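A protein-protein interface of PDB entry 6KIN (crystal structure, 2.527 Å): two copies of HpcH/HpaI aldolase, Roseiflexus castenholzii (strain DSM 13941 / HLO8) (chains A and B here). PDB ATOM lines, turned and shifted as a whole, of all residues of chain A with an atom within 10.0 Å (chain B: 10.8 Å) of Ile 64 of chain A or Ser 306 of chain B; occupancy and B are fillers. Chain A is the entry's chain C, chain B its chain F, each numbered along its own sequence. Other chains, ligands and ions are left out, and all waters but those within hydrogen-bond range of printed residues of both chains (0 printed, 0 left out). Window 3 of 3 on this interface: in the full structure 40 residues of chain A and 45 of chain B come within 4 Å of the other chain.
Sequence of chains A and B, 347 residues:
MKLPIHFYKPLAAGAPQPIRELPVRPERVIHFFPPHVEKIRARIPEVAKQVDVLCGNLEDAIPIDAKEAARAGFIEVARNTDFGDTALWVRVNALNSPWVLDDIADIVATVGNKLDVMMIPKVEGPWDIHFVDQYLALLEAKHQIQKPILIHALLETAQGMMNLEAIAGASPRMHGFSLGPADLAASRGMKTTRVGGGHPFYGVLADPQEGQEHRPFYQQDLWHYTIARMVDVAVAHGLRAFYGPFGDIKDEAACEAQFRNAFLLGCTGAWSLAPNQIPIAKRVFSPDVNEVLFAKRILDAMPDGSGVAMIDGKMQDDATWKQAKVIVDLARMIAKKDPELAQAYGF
OD2 of Asp 60 of chain A lies close to OD1 of Asp 317 of chain B (3.4 Å). N of Ile 64 of chain A is in hydrogen-bond range of OG of Ser 306 of chain B (3.1 Å). N of Ala 61 of chain A lies within hydrogen-bond range of OD1 of Asp 318 of chain B (3.1 Å).
OD1 of Asp 317 of chain B sits close to N of Ala 319 of chain B, at 3.3 Å. The side-chain carboxylate (OD1) of Asp 318 of chain B lies within hydrogen-bond range of the backbone NH (N) of Gly 307 of chain B. O of Asp 317 of chain B lies within hydrogen-bond range of OG1 of Thr 320 of chain B (3.0 Å). OD2 of Asp 304 of chain B lies within hydrogen-bond range of OG of Ser 306 of chain B (3.3 Å).
OD1 of Asp 60 of chain A touches CB of Asp 318 of chain B (3.3 Å). N of Ala 319 of chain B touches OD2 of Asp 60 of chain A, 3.6 Å away. Ala 61 of chain A touches Gly 307 of chain B. Ala 61 of chain A touches Val 308 of chain B (O to CG1, 3.7 Å). CB of Asp 317 of chain B touches CB of Ala 61 of chain A, at 3.8 Å. OG of Ser 306 of chain B touches CA of Pro 63 of chain A, 3.8 Å away. N of Pro 63 of chain A touches CA of Gly 307 of chain B, at 3.9 Å.
Ile 64 of chain A touches just one residue of chain B: Ser 306. Of the printed residues of chain A, Ser 306 of chain B touches Pro 63 (3.8 Å) and Ile 64 (3.1 Å). Pro 63 of chain A touches just these residues of chain B: Ser 306 and Gly 307. No residue of chain B comes within 4 Å of Asp 65 of chain A. No residue of chain B comes within 4 Å of Ala 66 of chain A. No residue of chain B comes within 4 Å of Lys 67 of chain A. No residue of chain A comes within 4 Å of Asp 304 of chain B. No residue of chain A comes within 4 Å of Gly 305 of chain B. Of the printed residues of chain A, Ala 319 of chain B touches Asp 60 (3.6 Å). Printed residues of chain B within 4 Å of Asp 60 of chain A: Asp 317 (3.2 Å), Asp 318 (3.3 Å) and Ala 319 (3.6 Å). Of the printed residues of chain B, Ala 61 of chain A touches Gly 307 (3.1 Å), Val 308 (3.7 Å), Asp 317 (3.8 Å) and Asp 318 (3.1 Å). Of the printed residues of chain A, Asp 318 of chain B touches Asp 60 (3.3 Å) and Ala 61 (3.1 Å). Printed residues of chain A within 4 Å of Asp 317 of chain B: Asp 60 and Ala 61. Gln 316 of chain B touches none of the printed residues of chain A. Ala 309 of chain B touches none of the printed residues of chain A. The nearest residue of chain A that does not touch Ser 306 of chain B is Ile 62 of chain A (4.1 Å). The nearest printed residue of chain B that does not touch Asp 60 of chain A is Lys 322 of chain B (4.3 Å).
Hydrophobic or aromatic side chains of chain B within 4 Å of the printed part of chain A: Val 308 and Ala 319. Printed residues of chain A that touch a printed residue of chain B: Asp 60, Ala 61, Pro 63 and Ile 64. Hydrophobic or aromatic side chains of chain A that line the printed part of chain B: Ala 61 and Ile 64. Among the printed residues, no Asp or Glu carboxylate lies within 4 Å of a Lys or Arg side-chain nitrogen of the other chain.
No position is printed for both chains.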
ATOM      1  N   HIS A  36     -24.552   6.292  22.844  1.00  0.00           N
ATOM      2  CA  HIS A  36     -25.990   6.537  23.131  1.00  0.00           C
ATOM      3  C   HIS A  36     -26.818   6.663  21.858  1.00  0.00           C
ATOM      4  O   HIS A  36     -28.014   6.806  21.973  1.00  0.00           O
ATOM      5  CB  HIS A  36     -26.153   7.794  23.978  1.00  0.00           C
ATOM      6  CG  HIS A  36     -25.691   9.037  23.316  1.00  0.00           C
ATOM      7  ND1 HIS A  36     -24.417   9.203  22.885  1.00  0.00           N
ATOM      8  CD2 HIS A  36     -26.329  10.174  23.014  1.00  0.00           C
ATOM      9  CE1 HIS A  36     -24.290  10.375  22.337  1.00  0.00           C
ATOM     10  NE2 HIS A  36     -25.436  10.982  22.403  1.00  0.00           N
ATOM     11  N   LEU A  58     -17.678   8.227  26.979  1.00  0.00           N
ATOM     12  CA  LEU A  58     -18.722   8.677  27.882  1.00  0.00           C
ATOM     13  C   LEU A  58     -18.532  10.092  28.401  1.00  0.00           C
ATOM     14  O   LEU A  58     -19.468  10.620  29.018  1.00  0.00           O
ATOM     15  CB  LEU A  58     -18.847   7.737  29.089  1.00  0.00           C
ATOM     16  CG  LEU A  58     -18.666   6.239  28.911  1.00  0.00           C
ATOM     17  CD1 LEU A  58     -18.683   5.553  30.266  1.00  0.00           C
ATOM     18  CD2 LEU A  58     -19.783   5.730  28.051  1.00  0.00           C
ATOM     19  N   GLU A  59     -17.364  10.714  28.178  1.00  0.00           N
ATOM     20  CA  GLU A  59     -17.033  12.024  28.735  1.00  0.00           C
ATOM     21  C   GLU A  59     -17.388  13.122  27.733  1.00  0.00           C
ATOM     22  O   GLU A  59     -18.557  13.292  27.384  1.00  0.00           O
ATOM     23  CB  GLU A  59     -15.535  12.078  29.120  1.00  0.00           C
ATOM     24  CG  GLU A  59     -15.148  13.165  30.126  1.00  0.00           C
ATOM     25  CD  GLU A  59     -13.958  14.047  29.668  1.00  0.00           C
ATOM     26  OE1 GLU A  59     -13.307  13.733  28.639  1.00  0.00           O
ATOM     27  OE2 GLU A  59     -13.664  15.064  30.351  1.00  0.00           O
ATOM     28  N   ASP A  60     -16.377  13.853  27.255  1.00  0.00           N
ATOM     29  CA  ASP A  60     -16.587  15.020  26.414  1.00  0.00           C
ATOM     30  C   ASP A  60     -17.280  14.632  25.115  1.00  0.00           C
ATOM     31  O   ASP A  60     -17.079  13.537  24.581  1.00  0.00           O
ATOM     32  CB  ASP A  60     -15.252  15.704  26.107  1.00  0.00           C
ATOM     33  CG  ASP A  60     -14.806  16.677  27.219  1.00  0.00           C
ATOM     34  OD1 ASP A  60     -15.492  16.724  28.279  1.00  0.00           O
ATOM     35  OD2 ASP A  60     -13.784  17.405  27.031  1.00  0.00           O
ATOM     36  N   ALA A  61     -18.097  15.561  24.603  1.00  0.00           N
ATOM     37  CA  ALA A  61     -18.959  15.446  23.416  1.00  0.00           C
ATOM     38  C   ALA A  61     -20.210  14.587  23.638  1.00  0.00           C
ATOM     39  O   ALA A  61     -20.976  14.408  22.682  1.00  0.00           O
ATOM     40  CB  ALA A  61     -18.210  14.905  22.188  1.00  0.00           C
ATOM     41  N   ILE A  62     -20.448  14.044  24.825  1.00  0.00           N
ATOM     42  CA  ILE A  62     -21.729  13.429  25.170  1.00  0.00           C
ATOM     43  C   ILE A  62     -22.546  14.473  25.924  1.00  0.00           C
ATOM     44  O   ILE A  62     -22.081  14.967  26.955  1.00  0.00           O
ATOM     45  CB  ILE A  62     -21.536  12.163  26.021  1.00  0.00           C
ATOM     46  CG1 ILE A  62     -20.563  11.177  25.333  1.00  0.00           C
ATOM     47  CG2 ILE A  62     -22.877  11.512  26.370  1.00  0.00           C
ATOM     48  CD1 ILE A  62     -21.158  10.349  24.220  1.00  0.00           C
ATOM     49  N   PRO A  63     -23.724  14.857  25.448  1.00  0.00           N
ATOM     50  CA  PRO A  63     -24.548  15.807  26.222  1.00  0.00           C
ATOM     51  C   PRO A  63     -24.783  15.288  27.633  1.00  0.00           C
ATOM     52  O   PRO A  63     -24.831  14.078  27.863  1.00  0.00           O
ATOM     53  CB  PRO A  63     -25.861  15.881  25.430  1.00  0.00           C
ATOM     54  CG  PRO A  63     -25.539  15.376  24.077  1.00  0.00           C
ATOM     55  CD  PRO A  63     -24.362  14.444  24.185  1.00  0.00           C
ATOM     56  N   ILE A  64     -24.928  16.221  28.583  1.00  0.00           N
ATOM     57  CA  ILE A  64     -25.162  15.849  29.983  1.00  0.00           C
ATOM     58  C   ILE A  64     -26.428  15.007  30.114  1.00  0.00           C
ATOM     59  O   ILE A  64     -26.482  14.060  30.909  1.00  0.00           O
ATOM     60  CB  ILE A  64     -25.215  17.113  30.867  1.00  0.00           C
ATOM     61  CG1 ILE A  64     -23.797  17.547  31.263  1.00  0.00           C
ATOM     62  CG2 ILE A  64     -26.048  16.880  32.109  1.00  0.00           C
ATOM     63  CD1 ILE A  64     -23.613  19.073  31.459  1.00  0.00           C
ATOM     64  N   ASP A  65     -27.414  15.291  29.289  1.00  0.00           N
ATOM     65  CA  ASP A  65     -28.697  14.552  29.296  1.00  0.00           C
ATOM     66  C   ASP A  65     -28.510  13.097  28.901  1.00  0.00           C
ATOM     67  O   ASP A  65     -29.340  12.289  29.247  1.00  0.00           O
ATOM     68  CB  ASP A  65     -29.604  15.057  28.190  1.00  0.00           C
ATOM     69  CG  ASP A  65     -30.155  16.427  28.465  1.00  0.00           C
ATOM     70  OD1 ASP A  65     -29.968  16.913  29.576  1.00  0.00           O
ATOM     71  OD2 ASP A  65     -30.780  16.982  27.563  1.00  0.00           O
ATOM     72  N   ALA A  66     -27.489  12.825  28.114  1.00  0.00           N
ATOM     73  CA  ALA A  66     -27.322  11.510  27.529  1.00  0.00           C
ATOM     74  C   ALA A  66     -26.301  10.645  28.262  1.00  0.00           C
ATOM     75  O   ALA A  66     -25.958   9.567  27.756  1.00  0.00           O
ATOM     76  CB  ALA A  66     -26.925  11.658  26.062  1.00  0.00           C
ATOM     77  N   LYS A  67     -25.817  11.075  29.438  1.00  0.00           N
ATOM     78  CA  LYS A  67     -24.709  10.367  30.084  1.00  0.00           C
ATOM     79  C   LYS A  67     -25.111   8.950  30.476  1.00  0.00           C
ATOM     80  O   LYS A  67     -24.426   7.980  30.128  1.00  0.00           O
ATOM     81  CB  LYS A  67     -24.210  11.137  31.312  1.00  0.00           C
ATOM     82  CG  LYS A  67     -23.532  12.464  31.004  1.00  0.00           C
ATOM     83  CD  LYS A  67     -22.218  12.306  30.263  1.00  0.00           C
ATOM     84  CE  LYS A  67     -21.405  13.585  30.338  1.00  0.00           C
ATOM     85  NZ  LYS A  67     -20.186  13.544  29.490  1.00  0.00           N
ATOM     86  N   GLU A  68     -26.225   8.809  31.196  1.00  0.00           N
ATOM     87  CA  GLU A  68     -26.694   7.483  31.591  1.00  0.00           C
ATOM     88  C   GLU A  68     -26.969   6.601  30.371  1.00  0.00           C
ATOM     89  O   GLU A  68     -26.697   5.392  30.393  1.00  0.00           O
ATOM     90  CB  GLU A  68     -27.942   7.621  32.464  1.00  0.00           C
ATOM     91  CG  GLU A  68     -27.695   8.308  33.824  1.00  0.00           C
ATOM     92  CD  GLU A  68     -27.588   9.852  33.754  1.00  0.00           C
ATOM     93  OE1 GLU A  68     -27.799  10.457  32.655  1.00  0.00           O
ATOM     94  OE2 GLU A  68     -27.297  10.454  34.829  1.00  0.00           O
ATOM     95  N   ALA A  69     -27.484   7.198  29.284  1.00  0.00           N
ATOM     96  CA  ALA A  69     -27.762   6.438  28.066  1.00  0.00           C
ATOM     97  C   ALA A  69     -26.483   5.952  27.400  1.00  0.00           C
ATOM     98  O   ALA A  69     -26.438   4.831  26.892  1.00  0.00           O
ATOM     99  CB  ALA A  69     -28.579   7.282  27.083  1.00  0.00           C
ATOM    100  N   ALA A  70     -25.435   6.781  27.375  1.00  0.00           N
ATOM    101  CA  ALA A  70     -24.186   6.343  26.764  1.00  0.00           C
ATOM    102  C   ALA A  70     -23.580   5.166  27.519  1.00  0.00           C
ATOM    103  O   ALA A  70     -22.924   4.308  26.914  1.00  0.00           O
ATOM    104  CB  ALA A  70     -23.194   7.503  26.693  1.00  0.00           C
ATOM    105  N   ARG A  71     -23.800   5.108  28.832  1.00  0.00           N
ATOM    106  CA  ARG A  71     -23.291   4.005  29.638  1.00  0.00           C
ATOM    107  C   ARG A  71     -24.023   2.710  29.315  1.00  0.00           C
ATOM    108  O   ARG A  71     -23.398   1.669  29.093  1.00  0.00           O
ATOM    109  CB  ARG A  71     -23.435   4.360  31.126  1.00  0.00           C
ATOM    110  CG  ARG A  71     -22.768   3.424  32.126  1.00  0.00           C
ATOM    111  CD  ARG A  71     -22.480   4.188  33.423  1.00  0.00           C
ATOM    112  NE  ARG A  71     -23.687   4.483  34.208  1.00  0.00           N
ATOM    113  CZ  ARG A  71     -23.803   5.462  35.106  1.00  0.00           C
ATOM    114  NH1 ARG A  71     -22.795   6.289  35.348  1.00  0.00           N
ATOM    115  NH2 ARG A  71     -24.942   5.623  35.764  1.00  0.00           N
ATOM    116  N   ASN A  93     -15.879   9.077  32.701  1.00  0.00           N
ATOM    117  CA  ASN A  93     -15.956  10.478  33.068  1.00  0.00           C
ATOM    118  C   ASN A  93     -14.842  10.855  34.046  1.00  0.00           C
ATOM    119  O   ASN A  93     -14.194  10.007  34.666  1.00  0.00           O
ATOM    120  CB  ASN A  93     -17.327  10.784  33.663  1.00  0.00           C
ATOM    121  CG  ASN A  93     -18.368  11.018  32.598  1.00  0.00           C
ATOM    122  OD1 ASN A  93     -18.408  12.082  31.962  1.00  0.00           O
ATOM    123  ND2 ASN A  93     -19.207  10.023  32.377  1.00  0.00           N
ATOM    124  N   SER A  97     -16.655  13.814  38.757  1.00  0.00           N
ATOM    125  CA  SER A  97     -17.960  13.918  38.134  1.00  0.00           C
ATOM    126  C   SER A  97     -18.969  13.022  38.834  1.00  0.00           C
ATOM    127  O   SER A  97     -18.603  12.073  39.536  1.00  0.00           O
ATOM    128  CB  SER A  97     -17.866  13.549  36.640  1.00  0.00           C
ATOM    129  OG  SER A  97     -17.509  12.192  36.473  1.00  0.00           O
ATOM    130  N   PRO A  98     -20.265  13.307  38.677  1.00  0.00           N
ATOM    131  CA  PRO A  98     -21.286  12.455  39.306  1.00  0.00           C
ATOM    132  C   PRO A  98     -21.481  11.116  38.617  1.00  0.00           C
ATOM    133  O   PRO A  98     -22.271  10.310  39.114  1.00  0.00           O
ATOM    134  CB  PRO A  98     -22.567  13.301  39.199  1.00  0.00           C
ATOM    135  CG  PRO A  98     -22.111  14.684  38.872  1.00  0.00           C
ATOM    136  CD  PRO A  98     -20.866  14.495  38.051  1.00  0.00           C
ATOM    137  N   TRP A  99     -20.804  10.844  37.490  1.00  0.00           N
ATOM    138  CA  TRP A  99     -21.028   9.607  36.756  1.00  0.00           C
ATOM    139  C   TRP A  99     -19.885   8.609  36.839  1.00  0.00           C
ATOM    140  O   TRP A  99     -20.093   7.439  36.493  1.00  0.00           O
ATOM    141  CB  TRP A  99     -21.328   9.896  35.278  1.00  0.00           C
ATOM    142  CG  TRP A  99     -22.337  10.980  35.100  1.00  0.00           C
ATOM    143  CD1 TRP A  99     -23.686  10.877  35.241  1.00  0.00           C
ATOM    144  CD2 TRP A  99     -22.070  12.341  34.770  1.00  0.00           C
ATOM    145  NE1 TRP A  99     -24.282  12.097  35.018  1.00  0.00           N
ATOM    146  CE2 TRP A  99     -23.309  13.012  34.724  1.00  0.00           C
ATOM    147  CE3 TRP A  99     -20.900  13.060  34.508  1.00  0.00           C
ATOM    148  CZ2 TRP A  99     -23.414  14.369  34.425  1.00  0.00           C
ATOM    149  CZ3 TRP A  99     -21.005  14.408  34.208  1.00  0.00           C
ATOM    150  CH2 TRP A  99     -22.257  15.051  34.176  1.00  0.00           C
ATOM    151  N   ILE B 298     -18.757  29.096  18.788  1.00  0.00           N
ATOM    152  CA  ILE B 298     -18.653  27.876  19.585  1.00  0.00           C
ATOM    153  C   ILE B 298     -19.517  27.978  20.841  1.00  0.00           C
ATOM    154  O   ILE B 298     -20.286  27.067  21.153  1.00  0.00           O
ATOM    155  CB  ILE B 298     -17.178  27.584  19.927  1.00  0.00           C
ATOM    156  CG1 ILE B 298     -16.345  27.488  18.641  1.00  0.00           C
ATOM    157  CG2 ILE B 298     -17.048  26.307  20.747  1.00  0.00           C
ATOM    158  CD1 ILE B 298     -14.864  27.252  18.854  1.00  0.00           C
ATOM    159  N   LEU B 299     -19.407  29.091  21.576  1.00  0.00           N
ATOM    160  CA  LEU B 299     -20.215  29.262  22.785  1.00  0.00           C
ATOM    161  C   LEU B 299     -21.699  29.164  22.494  1.00  0.00           C
ATOM    162  O   LEU B 299     -22.466  28.699  23.345  1.00  0.00           O
ATOM    163  CB  LEU B 299     -19.927  30.608  23.452  1.00  0.00           C
ATOM    164  CG  LEU B 299     -18.532  30.766  24.050  1.00  0.00           C
ATOM    165  CD1 LEU B 299     -18.351  32.164  24.589  1.00  0.00           C
ATOM    166  CD2 LEU B 299     -18.275  29.700  25.114  1.00  0.00           C
ATOM    167  N   ASP B 300     -22.126  29.619  21.312  1.00  0.00           N
ATOM    168  CA  ASP B 300     -23.547  29.593  20.988  1.00  0.00           C
ATOM    169  C   ASP B 300     -24.017  28.170  20.729  1.00  0.00           C
ATOM    170  O   ASP B 300     -25.093  27.771  21.190  1.00  0.00           O
ATOM    171  CB  ASP B 300     -23.830  30.474  19.770  1.00  0.00           C
ATOM    172  CG  ASP B 300     -23.543  31.956  20.018  1.00  0.00           C
ATOM    173  OD1 ASP B 300     -23.428  32.369  21.203  1.00  0.00           O
ATOM    174  OD2 ASP B 300     -23.424  32.704  19.007  1.00  0.00           O
ATOM    175  N   ALA B 301     -23.195  27.379  20.033  1.00  0.00           N
ATOM    176  CA  ALA B 301     -23.610  26.060  19.566  1.00  0.00           C
ATOM    177  C   ALA B 301     -23.841  25.057  20.700  1.00  0.00           C
ATOM    178  O   ALA B 301     -24.508  24.045  20.471  1.00  0.00           O
ATOM    179  CB  ALA B 301     -22.574  25.531  18.573  1.00  0.00           C
ATOM    180  N   MET B 302     -23.316  25.307  21.905  1.00  0.00           N
ATOM    181  CA  MET B 302     -23.545  24.432  23.064  1.00  0.00           C
ATOM    182  C   MET B 302     -23.620  25.270  24.334  1.00  0.00           C
ATOM    183  O   MET B 302     -22.659  25.336  25.111  1.00  0.00           O
ATOM    184  CB  MET B 302     -22.440  23.384  23.219  1.00  0.00           C
ATOM    185  CG  MET B 302     -21.962  22.674  21.970  1.00  0.00           C
ATOM    186  SD  MET B 302     -20.260  22.076  22.190  1.00  0.00           S
ATOM    187  CE  MET B 302     -19.342  23.452  21.479  1.00  0.00           C
ATOM    188  N   PRO B 303     -24.768  25.910  24.597  1.00  0.00           N
ATOM    189  CA  PRO B 303     -24.839  26.842  25.742  1.00  0.00           C
ATOM    190  C   PRO B 303     -24.521  26.196  27.079  1.00  0.00           C
ATOM    191  O   PRO B 303     -23.905  26.842  27.934  1.00  0.00           O
ATOM    192  CB  PRO B 303     -26.287  27.353  25.691  1.00  0.00           C
ATOM    193  CG  PRO B 303     -26.738  27.098  24.283  1.00  0.00           C
ATOM    194  CD  PRO B 303     -26.048  25.826  23.876  1.00  0.00           C
ATOM    195  N   ASP B 304     -24.915  24.937  27.282  1.00  0.00           N
ATOM    196  CA  ASP B 304     -24.577  24.195  28.496  1.00  0.00           C
ATOM    197  C   ASP B 304     -23.094  23.833  28.572  1.00  0.00           C
ATOM    198  O   ASP B 304     -22.657  23.262  29.584  1.00  0.00           O
ATOM    199  CB  ASP B 304     -25.428  22.913  28.585  1.00  0.00           C
ATOM    200  CG  ASP B 304     -25.248  21.997  27.376  1.00  0.00           C
ATOM    201  OD1 ASP B 304     -24.703  22.448  26.330  1.00  0.00           O
ATOM    202  OD2 ASP B 304     -25.656  20.813  27.468  1.00  0.00           O
ATOM    203  N   GLY B 305     -22.322  24.128  27.524  1.00  0.00           N
ATOM    204  CA  GLY B 305     -20.922  23.750  27.446  1.00  0.00           C
ATOM    205  C   GLY B 305     -20.633  22.269  27.322  1.00  0.00           C
ATOM    206  O   GLY B 305     -19.480  21.868  27.510  1.00  0.00           O
ATOM    207  N   SER B 306     -21.635  21.442  27.015  1.00  0.00           N
ATOM    208  CA  SER B 306     -21.442  20.000  26.907  1.00  0.00           C
ATOM    209  C   SER B 306     -22.237  19.462  25.721  1.00  0.00           C
ATOM    210  O   SER B 306     -23.389  19.852  25.508  1.00  0.00           O
ATOM    211  CB  SER B 306     -21.845  19.283  28.210  1.00  0.00           C
ATOM    212  OG  SER B 306     -23.165  18.775  28.151  1.00  0.00           O
ATOM    213  N   GLY B 307     -21.615  18.566  24.948  1.00  0.00           N
ATOM    214  CA  GLY B 307     -22.212  18.006  23.758  1.00  0.00           C
ATOM    215  C   GLY B 307     -21.251  18.117  22.596  1.00  0.00           C
ATOM    216  O   GLY B 307     -20.038  18.260  22.782  1.00  0.00           O
ATOM    217  N   VAL B 308     -21.796  18.086  21.380  1.00  0.00           N
ATOM    218  CA  VAL B 308     -20.992  18.068  20.167  1.00  0.00           C
ATOM    219  C   VAL B 308     -21.626  18.990  19.128  1.00  0.00           C
ATOM    220  O   VAL B 308     -22.832  19.244  19.156  1.00  0.00           O
ATOM    221  CB  VAL B 308     -20.825  16.606  19.661  1.00  0.00           C
ATOM    222  CG1 VAL B 308     -22.173  15.884  19.557  1.00  0.00           C
ATOM    223  CG2 VAL B 308     -20.017  16.529  18.363  1.00  0.00           C
ATOM    224  N   ALA B 309     -20.794  19.542  18.242  1.00  0.00           N
ATOM    225  CA  ALA B 309     -21.281  20.373  17.141  1.00  0.00           C
ATOM    226  C   ALA B 309     -20.235  20.381  16.038  1.00  0.00           C
ATOM    227  O   ALA B 309     -19.082  19.990  16.246  1.00  0.00           O
ATOM    228  CB  ALA B 309     -21.604  21.809  17.578  1.00  0.00           C
ATOM    229  N   GLN B 316     -16.699  20.292  17.525  1.00  0.00           N
ATOM    230  CA  GLN B 316     -16.699  21.022  18.787  1.00  0.00           C
ATOM    231  C   GLN B 316     -17.274  20.145  19.899  1.00  0.00           C
ATOM    232  O   GLN B 316     -18.236  19.396  19.683  1.00  0.00           O
ATOM    233  CB  GLN B 316     -17.518  22.325  18.687  1.00  0.00           C
ATOM    234  CG  GLN B 316     -17.267  23.155  17.438  1.00  0.00           C
ATOM    235  CD  GLN B 316     -15.851  23.715  17.372  1.00  0.00           C
ATOM    236  OE1 GLN B 316     -15.266  24.102  18.386  1.00  0.00           O
ATOM    237  NE2 GLN B 316     -15.286  23.729  16.172  1.00  0.00           N
ATOM    238  N   ASP B 317     -16.682  20.256  21.089  1.00  0.00           N
ATOM    239  CA  ASP B 317     -17.089  19.505  22.272  1.00  0.00           C
ATOM    240  C   ASP B 317     -16.887  20.393  23.500  1.00  0.00           C
ATOM    241  O   ASP B 317     -16.634  21.598  23.384  1.00  0.00           O
ATOM    242  CB  ASP B 317     -16.307  18.185  22.357  1.00  0.00           C
ATOM    243  CG  ASP B 317     -14.832  18.379  22.769  1.00  0.00           C
ATOM    244  OD1 ASP B 317     -14.358  17.642  23.662  1.00  0.00           O
ATOM    245  OD2 ASP B 317     -14.129  19.251  22.200  1.00  0.00           O
ATOM    246  N   ASP B 318     -17.006  19.792  24.690  1.00  0.00           N
ATOM    247  CA  ASP B 318     -16.700  20.502  25.933  1.00  0.00           C
ATOM    248  C   ASP B 318     -15.345  21.207  25.872  1.00  0.00           C
ATOM    249  O   ASP B 318     -15.215  22.356  26.311  1.00  0.00           O
ATOM    250  CB  ASP B 318     -16.722  19.531  27.117  1.00  0.00           C
ATOM    251  CG  ASP B 318     -18.020  18.751  27.210  1.00  0.00           C
ATOM    252  OD1 ASP B 318     -18.485  18.262  26.156  1.00  0.00           O
ATOM    253  OD2 ASP B 318     -18.585  18.637  28.320  1.00  0.00           O
ATOM    254  N   ALA B 319     -14.324  20.535  25.319  1.00  0.00           N
ATOM    255  CA  ALA B 319     -12.968  21.075  25.370  1.00  0.00           C
ATOM    256  C   ALA B 319     -12.825  22.338  24.524  1.00  0.00           C
ATOM    257  O   ALA B 319     -12.178  23.301  24.952  1.00  0.00           O
ATOM    258  CB  ALA B 319     -11.959  20.019  24.929  1.00  0.00           C
ATOM    259  N   THR B 320     -13.408  22.359  23.318  1.00  0.00           N
ATOM    260  CA  THR B 320     -13.375  23.587  22.523  1.00  0.00           C
ATOM    261  C   THR B 320     -14.266  24.666  23.125  1.00  0.00           C
ATOM    262  O   THR B 320     -13.999  25.861  22.944  1.00  0.00           O
ATOM    263  CB  THR B 320     -13.804  23.327  21.085  1.00  0.00           C
ATOM    264  OG1 THR B 320     -15.178  22.911  21.073  1.00  0.00           O
ATOM    265  CG2 THR B 320     -12.913  22.268  20.426  1.00  0.00           C
ATOM    266  N   TRP B 321     -15.332  24.274  23.825  1.00  0.00           N
ATOM    267  CA  TRP B 321     -16.131  25.259  24.541  1.00  0.00           C
ATOM    268  C   TRP B 321     -15.280  25.991  25.569  1.00  0.00           C
ATOM    269  O   TRP B 321     -15.341  27.221  25.667  1.00  0.00           O
ATOM    270  CB  TRP B 321     -17.336  24.588  25.198  1.00  0.00           C
ATOM    271  CG  TRP B 321     -18.384  25.553  25.700  1.00  0.00           C
ATOM    272  CD1 TRP B 321     -19.476  26.020  25.012  1.00  0.00           C
ATOM    273  CD2 TRP B 321     -18.440  26.168  27.002  1.00  0.00           C
ATOM    274  NE1 TRP B 321     -20.201  26.877  25.809  1.00  0.00           N
ATOM    275  CE2 TRP B 321     -19.590  26.983  27.030  1.00  0.00           C
ATOM    276  CE3 TRP B 321     -17.632  26.102  28.141  1.00  0.00           C
ATOM    277  CZ2 TRP B 321     -19.949  27.725  28.150  1.00  0.00           C
ATOM    278  CZ3 TRP B 321     -17.989  26.838  29.253  1.00  0.00           C
ATOM    279  CH2 TRP B 321     -19.138  27.641  29.250  1.00  0.00           C
ATOM    280  N   LYS B 322     -14.451  25.252  26.320  1.00  0.00           N
ATOM    281  CA  LYS B 322     -13.566  25.871  27.310  1.00  0.00           C
ATOM    282  C   LYS B 322     -12.447  26.676  26.654  1.00  0.00           C
ATOM    283  O   LYS B 322     -11.920  27.619  27.259  1.00  0.00           O
ATOM    284  CB  LYS B 322     -12.969  24.803  28.230  1.00  0.00           C
ATOM    285  CG  LYS B 322     -13.987  23.915  28.921  1.00  0.00           C
ATOM    286  CD  LYS B 322     -13.307  22.830  29.754  1.00  0.00           C
ATOM    287  CE  LYS B 322     -14.330  21.933  30.456  1.00  0.00           C
ATOM    288  NZ  LYS B 322     -14.273  20.543  29.933  1.00  0.00           N
ATOM    289  N   LYS B 325     -14.258  29.910  25.906  1.00  0.00           N
ATOM    290  CA  LYS B 325     -14.497  30.698  27.112  1.00  0.00           C
ATOM    291  C   LYS B 325     -13.240  31.462  27.532  1.00  0.00           C
ATOM    292  O   LYS B 325     -13.320  32.640  27.901  1.00  0.00           O
ATOM    293  CB  LYS B 325     -14.997  29.807  28.246  1.00  0.00           C
ATOM    294  CG  LYS B 325     -15.474  30.604  29.444  1.00  0.00           C
ATOM    295  CD  LYS B 325     -15.559  29.741  30.701  1.00  0.00           C
ATOM    296  CE  LYS B 325     -15.520  30.578  31.976  1.00  0.00           C
ATOM    297  NZ  LYS B 325     -16.112  29.807  33.119  1.00  0.00           N
